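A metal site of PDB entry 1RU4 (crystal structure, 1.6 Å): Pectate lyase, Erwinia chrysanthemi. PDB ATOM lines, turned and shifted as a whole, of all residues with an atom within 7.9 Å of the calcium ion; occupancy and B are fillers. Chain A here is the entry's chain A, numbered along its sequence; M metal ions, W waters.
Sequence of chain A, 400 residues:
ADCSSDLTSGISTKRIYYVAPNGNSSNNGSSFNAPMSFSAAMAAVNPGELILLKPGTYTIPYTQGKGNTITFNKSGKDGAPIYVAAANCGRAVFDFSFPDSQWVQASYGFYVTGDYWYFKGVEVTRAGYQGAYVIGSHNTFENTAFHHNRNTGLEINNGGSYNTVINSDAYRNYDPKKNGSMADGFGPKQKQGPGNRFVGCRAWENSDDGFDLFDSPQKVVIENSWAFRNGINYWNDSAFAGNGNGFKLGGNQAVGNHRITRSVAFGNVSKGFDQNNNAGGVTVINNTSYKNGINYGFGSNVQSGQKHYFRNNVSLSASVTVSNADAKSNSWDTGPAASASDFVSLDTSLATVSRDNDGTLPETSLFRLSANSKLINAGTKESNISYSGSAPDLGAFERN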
ATOM      1  N   THR A 152      -7.019  -9.526  19.212  1.00  0.00           N
ATOM      2  CA  THR A 152      -6.077  -8.441  18.942  1.00  0.00           C
ATOM      3  C   THR A 152      -6.231  -7.235  19.878  1.00  0.00           C
ATOM      4  O   THR A 152      -7.350  -6.775  20.137  1.00  0.00           O
ATOM      5  CB  THR A 152      -6.167  -8.009  17.465  1.00  0.00           C
ATOM      6  OG1 THR A 152      -5.782  -9.116  16.635  1.00  0.00           O
ATOM      7  CG2 THR A 152      -5.269  -6.805  17.165  1.00  0.00           C
ATOM      8  N   GLY A 180      -4.774 -19.104  19.279  1.00  0.00           N
ATOM      9  CA  GLY A 180      -3.691 -18.135  19.206  1.00  0.00           C
ATOM     10  C   GLY A 180      -3.292 -17.667  17.826  1.00  0.00           C
ATOM     11  O   GLY A 180      -2.429 -16.798  17.699  1.00  0.00           O
ATOM     12  N   SER A 181      -3.926 -18.203  16.787  1.00  0.00           N
ATOM     13  CA  SER A 181      -3.581 -17.852  15.418  1.00  0.00           C
ATOM     14  C   SER A 181      -4.245 -16.578  14.887  1.00  0.00           C
ATOM     15  O   SER A 181      -4.172 -16.287  13.701  1.00  0.00           O
ATOM     16  CB  SER A 181      -3.879 -19.018  14.469  1.00  0.00           C
ATOM     17  OG  SER A 181      -5.274 -19.254  14.339  1.00  0.00           O
ATOM     18  N   MET A 182      -4.860 -15.804  15.778  1.00  0.00           N
ATOM     19  CA  MET A 182      -5.544 -14.588  15.358  1.00  0.00           C
ATOM     20  C   MET A 182      -5.127 -13.320  16.118  1.00  0.00           C
ATOM     21  O   MET A 182      -4.984 -12.253  15.517  1.00  0.00           O
ATOM     22  CB  MET A 182      -7.067 -14.782  15.487  1.00  0.00           C
ATOM     23  CG  MET A 182      -7.910 -13.728  14.799  1.00  0.00           C
ATOM     24  SD  MET A 182      -9.651 -14.209  14.786  1.00  0.00           S
ATOM     25  CE  MET A 182     -10.432 -12.636  14.920  1.00  0.00           C
ATOM     26  N   ALA A 183      -4.896 -13.448  17.420  1.00  0.00           N
ATOM     27  CA  ALA A 183      -4.606 -12.295  18.277  1.00  0.00           C
ATOM     28  C   ALA A 183      -3.242 -11.636  18.073  1.00  0.00           C
ATOM     29  O   ALA A 183      -2.204 -12.224  18.341  1.00  0.00           O
ATOM     30  CB  ALA A 183      -4.792 -12.669  19.732  1.00  0.00           C
ATOM     31  N   ASP A 184      -3.290 -10.388  17.619  1.00  0.00           N
ATOM     32  CA  ASP A 184      -2.086  -9.582  17.396  1.00  0.00           C
ATOM     33  C   ASP A 184      -1.984  -8.486  18.453  1.00  0.00           C
ATOM     34  O   ASP A 184      -2.859  -8.347  19.307  1.00  0.00           O
ATOM     35  CB  ASP A 184      -2.140  -8.922  16.020  1.00  0.00           C
ATOM     36  CG  ASP A 184      -2.298  -9.924  14.908  1.00  0.00           C
ATOM     37  OD1 ASP A 184      -3.138  -9.712  14.018  1.00  0.00           O
ATOM     38  OD2 ASP A 184      -1.577 -10.941  14.954  1.00  0.00           O
ATOM     39  N   GLY A 185      -0.901  -7.722  18.401  1.00  0.00           N
ATOM     40  CA  GLY A 185      -0.780  -6.573  19.265  1.00  0.00           C
ATOM     41  C   GLY A 185      -1.594  -5.446  18.661  1.00  0.00           C
ATOM     42  O   GLY A 185      -2.603  -5.010  19.221  1.00  0.00           O
ATOM     43  N   PHE A 186      -1.167  -4.987  17.487  1.00  0.00           N
ATOM     44  CA  PHE A 186      -1.859  -3.942  16.741  1.00  0.00           C
ATOM     45  C   PHE A 186      -2.264  -4.453  15.369  1.00  0.00           C
ATOM     46  O   PHE A 186      -1.462  -5.059  14.665  1.00  0.00           O
ATOM     47  CB  PHE A 186      -0.955  -2.718  16.593  1.00  0.00           C
ATOM     48  CG  PHE A 186      -0.621  -2.044  17.897  1.00  0.00           C
ATOM     49  CD1 PHE A 186       0.652  -2.149  18.437  1.00  0.00           C
ATOM     50  CD2 PHE A 186      -1.598  -1.309  18.577  1.00  0.00           C
ATOM     51  CE1 PHE A 186       0.961  -1.528  19.649  1.00  0.00           C
ATOM     52  CE2 PHE A 186      -1.289  -0.687  19.789  1.00  0.00           C
ATOM     53  CZ  PHE A 186      -0.013  -0.801  20.332  1.00  0.00           C
ATOM     54  N   GLY A 187      -3.509  -4.181  14.990  1.00  0.00           N
ATOM     55  CA  GLY A 187      -4.025  -4.702  13.738  1.00  0.00           C
ATOM     56  C   GLY A 187      -4.649  -3.741  12.741  1.00  0.00           C
ATOM     57  O   GLY A 187      -5.875  -3.744  12.586  1.00  0.00           O
ATOM     58  N   LYS A 189      -5.615  -3.391   9.589  1.00  0.00           N
ATOM     59  CA  LYS A 189      -5.708  -4.394   8.535  1.00  0.00           C
ATOM     60  C   LYS A 189      -7.020  -4.398   7.752  1.00  0.00           C
ATOM     61  O   LYS A 189      -7.950  -3.638   8.030  1.00  0.00           O
ATOM     62  CB  LYS A 189      -5.522  -5.782   9.151  1.00  0.00           C
ATOM     63  CG  LYS A 189      -6.609  -6.133  10.179  1.00  0.00           C
ATOM     64  CD  LYS A 189      -6.518  -7.555  10.701  1.00  0.00           C
ATOM     65  CE  LYS A 189      -5.303  -7.776  11.587  1.00  0.00           C
ATOM     66  NZ  LYS A 189      -5.342  -9.131  12.214  1.00  0.00           N
ATOM     67  N   SER A 207       0.018 -13.784  20.860  1.00  0.00           N
ATOM     68  CA  SER A 207       0.034 -15.146  20.338  1.00  0.00           C
ATOM     69  C   SER A 207       0.367 -15.233  18.851  1.00  0.00           C
ATOM     70  O   SER A 207       1.106 -16.121  18.438  1.00  0.00           O
ATOM     71  CB  SER A 207      -1.285 -15.863  20.648  1.00  0.00           C
ATOM     72  OG  SER A 207      -2.392 -15.219  20.030  1.00  0.00           O
ATOM     73  N   ASP A 208      -0.140 -14.292  18.060  1.00  0.00           N
ATOM     74  CA  ASP A 208       0.087 -14.320  16.629  1.00  0.00           C
ATOM     75  C   ASP A 208       1.207 -13.384  16.191  1.00  0.00           C
ATOM     76  O   ASP A 208       2.375 -13.785  16.213  1.00  0.00           O
ATOM     77  CB  ASP A 208      -1.215 -14.028  15.881  1.00  0.00           C
ATOM     78  CG  ASP A 208      -1.268 -14.659  14.496  1.00  0.00           C
ATOM     79  OD1 ASP A 208      -0.600 -15.690  14.268  1.00  0.00           O
ATOM     80  OD2 ASP A 208      -2.003 -14.147  13.648  1.00  0.00           O
ATOM     81  N   ASP A 209       0.880 -12.150  15.830  1.00  0.00           N
ATOM     82  CA  ASP A 209       1.895 -11.189  15.385  1.00  0.00           C
ATOM     83  C   ASP A 209       1.930  -9.920  16.235  1.00  0.00           C
ATOM     84  O   ASP A 209       0.960  -9.616  16.923  1.00  0.00           O
ATOM     85  CB  ASP A 209       1.642 -10.778  13.920  1.00  0.00           C
ATOM     86  CG  ASP A 209       1.438 -11.964  13.007  1.00  0.00           C
ATOM     87  OD1 ASP A 209       0.343 -12.086  12.429  1.00  0.00           O
ATOM     88  OD2 ASP A 209       2.370 -12.782  12.853  1.00  0.00           O
ATOM     89  N   GLY A 210       3.033  -9.182  16.151  1.00  0.00           N
ATOM     90  CA  GLY A 210       3.130  -7.916  16.860  1.00  0.00           C
ATOM     91  C   GLY A 210       2.231  -6.883  16.204  1.00  0.00           C
ATOM     92  O   GLY A 210       1.323  -6.341  16.834  1.00  0.00           O
ATOM     93  N   PHE A 211       2.500  -6.608  14.925  1.00  0.00           N
ATOM     94  CA  PHE A 211       1.694  -5.722  14.102  1.00  0.00           C
ATOM     95  C   PHE A 211       1.256  -6.545  12.898  1.00  0.00           C
ATOM     96  O   PHE A 211       2.062  -7.300  12.345  1.00  0.00           O
ATOM     97  CB  PHE A 211       2.518  -4.533  13.579  1.00  0.00           C
ATOM     98  CG  PHE A 211       2.922  -3.536  14.642  1.00  0.00           C
ATOM     99  CD1 PHE A 211       3.881  -3.870  15.602  1.00  0.00           C
ATOM    100  CD2 PHE A 211       2.392  -2.254  14.637  1.00  0.00           C
ATOM    101  CE1 PHE A 211       4.299  -2.920  16.544  1.00  0.00           C
ATOM    102  CE2 PHE A 211       2.808  -1.298  15.567  1.00  0.00           C
ATOM    103  CZ  PHE A 211       3.758  -1.636  16.527  1.00  0.00           C
ATOM    104  N   ASP A 212       0.004  -6.403  12.474  1.00  0.00           N
ATOM    105  CA  ASP A 212      -0.511  -7.157  11.326  1.00  0.00           C
ATOM    106  C   ASP A 212      -1.335  -6.256  10.402  1.00  0.00           C
ATOM    107  O   ASP A 212      -2.364  -5.715  10.801  1.00  0.00           O
ATOM    108  CB  ASP A 212      -1.358  -8.344  11.815  1.00  0.00           C
ATOM    109  CG  ASP A 212      -1.787  -9.276  10.676  1.00  0.00           C
ATOM    110  OD1 ASP A 212      -1.594  -8.962   9.493  1.00  0.00           O
ATOM    111  OD2 ASP A 212      -2.325 -10.356  10.982  1.00  0.00           O
ATOM    112  N   LEU A 213      -0.865  -6.151   9.162  1.00  0.00           N
ATOM    113  CA  LEU A 213      -1.482  -5.299   8.136  1.00  0.00           C
ATOM    114  C   LEU A 213      -2.120  -6.124   7.009  1.00  0.00           C
ATOM    115  O   LEU A 213      -2.272  -5.650   5.881  1.00  0.00           O
ATOM    116  CB  LEU A 213      -0.420  -4.359   7.544  1.00  0.00           C
ATOM    117  CG  LEU A 213       0.095  -3.181   8.394  1.00  0.00           C
ATOM    118  CD1 LEU A 213       0.639  -3.640   9.732  1.00  0.00           C
ATOM    119  CD2 LEU A 213       1.178  -2.454   7.617  1.00  0.00           C
ATOM    120  N   PHE A 214      -2.554  -7.342   7.356  1.00  0.00           N
ATOM    121  CA  PHE A 214      -3.124  -8.313   6.417  1.00  0.00           C
ATOM    122  C   PHE A 214      -4.213  -7.797   5.473  1.00  0.00           C
ATOM    123  O   PHE A 214      -5.191  -7.191   5.909  1.00  0.00           O
ATOM    124  CB  PHE A 214      -3.679  -9.498   7.216  1.00  0.00           C
ATOM    125  CG  PHE A 214      -4.199 -10.630   6.373  1.00  0.00           C
ATOM    126  CD1 PHE A 214      -3.324 -11.576   5.844  1.00  0.00           C
ATOM    127  CD2 PHE A 214      -5.555 -10.777   6.135  1.00  0.00           C
ATOM    128  CE1 PHE A 214      -3.793 -12.640   5.079  1.00  0.00           C
ATOM    129  CE2 PHE A 214      -6.047 -11.836   5.377  1.00  0.00           C
ATOM    130  CZ  PHE A 214      -5.163 -12.775   4.857  1.00  0.00           C
ATOM    131  N   ASN A 243       1.457 -17.579  14.739  1.00  0.00           N
ATOM    132  CA  ASN A 243       2.482 -17.469  13.697  1.00  0.00           C
ATOM    133  C   ASN A 243       3.815 -16.896  14.158  1.00  0.00           C
ATOM    134  O   ASN A 243       4.877 -17.354  13.737  1.00  0.00           O
ATOM    135  CB  ASN A 243       1.938 -16.682  12.499  1.00  0.00           C
ATOM    136  CG  ASN A 243       0.892 -17.448  11.724  1.00  0.00           C
ATOM    137  OD1 ASN A 243       1.131 -18.568  11.274  1.00  0.00           O
ATOM    138  ND2 ASN A 243      -0.285 -16.851  11.567  1.00  0.00           N
ATOM    139  N   GLY A 244       3.765 -15.863  15.000  1.00  0.00           N
ATOM    140  CA  GLY A 244       4.981 -15.313  15.583  1.00  0.00           C
ATOM    141  C   GLY A 244       5.831 -14.357  14.778  1.00  0.00           C
ATOM    142  O   GLY A 244       7.060 -14.426  14.850  1.00  0.00           O
ATOM    143  N   ASN A 245       5.213 -13.457  14.021  1.00  0.00           N
ATOM    144  CA  ASN A 245       5.981 -12.445  13.305  1.00  0.00           C
ATOM    145  C   ASN A 245       5.978 -11.135  14.086  1.00  0.00           C
ATOM    146  O   ASN A 245       5.043 -10.862  14.840  1.00  0.00           O
ATOM    147  CB  ASN A 245       5.417 -12.228  11.903  1.00  0.00           C
ATOM    148  CG  ASN A 245       5.363 -13.501  11.095  1.00  0.00           C
ATOM    149  OD1 ASN A 245       6.369 -13.956  10.551  1.00  0.00           O
ATOM    150  ND2 ASN A 245       4.179 -14.112  11.017  1.00  0.00           N
ATOM    151  N   LYS A 248       4.201  -7.893  10.636  1.00  0.00           N
ATOM    152  CA  LYS A 248       3.611  -8.557   9.473  1.00  0.00           C
ATOM    153  C   LYS A 248       3.076  -7.457   8.556  1.00  0.00           C
ATOM    154  O   LYS A 248       1.983  -6.927   8.763  1.00  0.00           O
ATOM    155  CB  LYS A 248       2.485  -9.508   9.905  1.00  0.00           C
ATOM    156  CG  LYS A 248       1.699 -10.101   8.733  1.00  0.00           C
ATOM    157  CD  LYS A 248       0.760 -11.213   9.180  1.00  0.00           C
ATOM    158  CE  LYS A 248       1.512 -12.508   9.430  1.00  0.00           C
ATOM    159  NZ  LYS A 248       0.616 -13.558   9.978  1.00  0.00           N
ATOM    160  N   ASN A 276       4.928 -11.155   4.126  1.00  0.00           N
ATOM    161  CA  ASN A 276       3.670 -11.908   4.169  1.00  0.00           C
ATOM    162  C   ASN A 276       2.844 -11.815   2.886  1.00  0.00           C
ATOM    163  O   ASN A 276       1.642 -11.521   2.914  1.00  0.00           O
ATOM    164  CB  ASN A 276       2.817 -11.516   5.376  1.00  0.00           C
ATOM    165  CG  ASN A 276       1.730 -12.522   5.671  1.00  0.00           C
ATOM    166  OD1 ASN A 276       1.965 -13.726   5.667  1.00  0.00           O
ATOM    167  ND2 ASN A 276       0.513 -12.028   5.910  1.00  0.00           N
HETATM  168 CA    CA M   1      -2.062 -11.860  12.839  1.00  0.00          CA
HETATM  169  O   HOH W   1      -4.605 -12.208  12.868  1.00  0.00           O
HETATM  170  O   HOH W   2      -2.430 -13.704  10.906  1.00  0.00           O
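O of Ala 183 lies within hydrogen-bond range of N of Asp 208 (2.9 Å).
O of Met 182 sits at hydrogen-bond distance from OG1 of Thr 152 (3.4 Å).
The side-chain amino group (NZ) of Lys 248 is in salt-bridge range of the side-chain carboxylate (OD2) of Asp 209, at 3.5 Å.
OG1 of Thr 152 sits at hydrogen-bond distance from N of Asp 184 (3.0 Å).
The side-chain carboxylate of Asp 212 sits at hydrogen-bond distance from the backbone NH of Phe 214 (2.8 Å).
N of Asp 208 sits at hydrogen-bond distance from O of Gly 180 (3.4 Å).
The backbone NH (N) of Asp 212 lies within hydrogen-bond range of the backbone carbonyl oxygen (O) of Phe 186, at 3.0 Å.
The backbone NH (N) of Gly 185 sits at hydrogen-bond distance from the backbone carbonyl oxygen (O) of Asp 209.
Residues that only touch the calcium ion: Met 182 (3.98 Å).
Five residues have an atom within 4 Å of the calcium ion: Met 182, Asp 184, Asp 208, Asp 209 and Asp 212.
The nearest printed residue that does not touch the calcium ion is Lys 248 (4.3 Å).
OD2 of Asp 184 binds the calcium ion, at 2.4 Å.
OD2 of Asp 212 binds the calcium ion (2.4 Å).
The side-chain carboxylate (OD2) of Asp 208 binds the calcium ion (2.4 Å).
The calcium ion is bound by OD1 of Asp 209, 2.5 Å away.
Water W1 is bound to the calcium ion.
OD1 of Asp 184 binds the calcium ion, at 2.7 Å.
The calcium ion is bound by water W2, 2.7 Å away.
Water W1 bridges the backbone carbonyl oxygen of Met 182 and the side-chain amino group of Lys 189.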
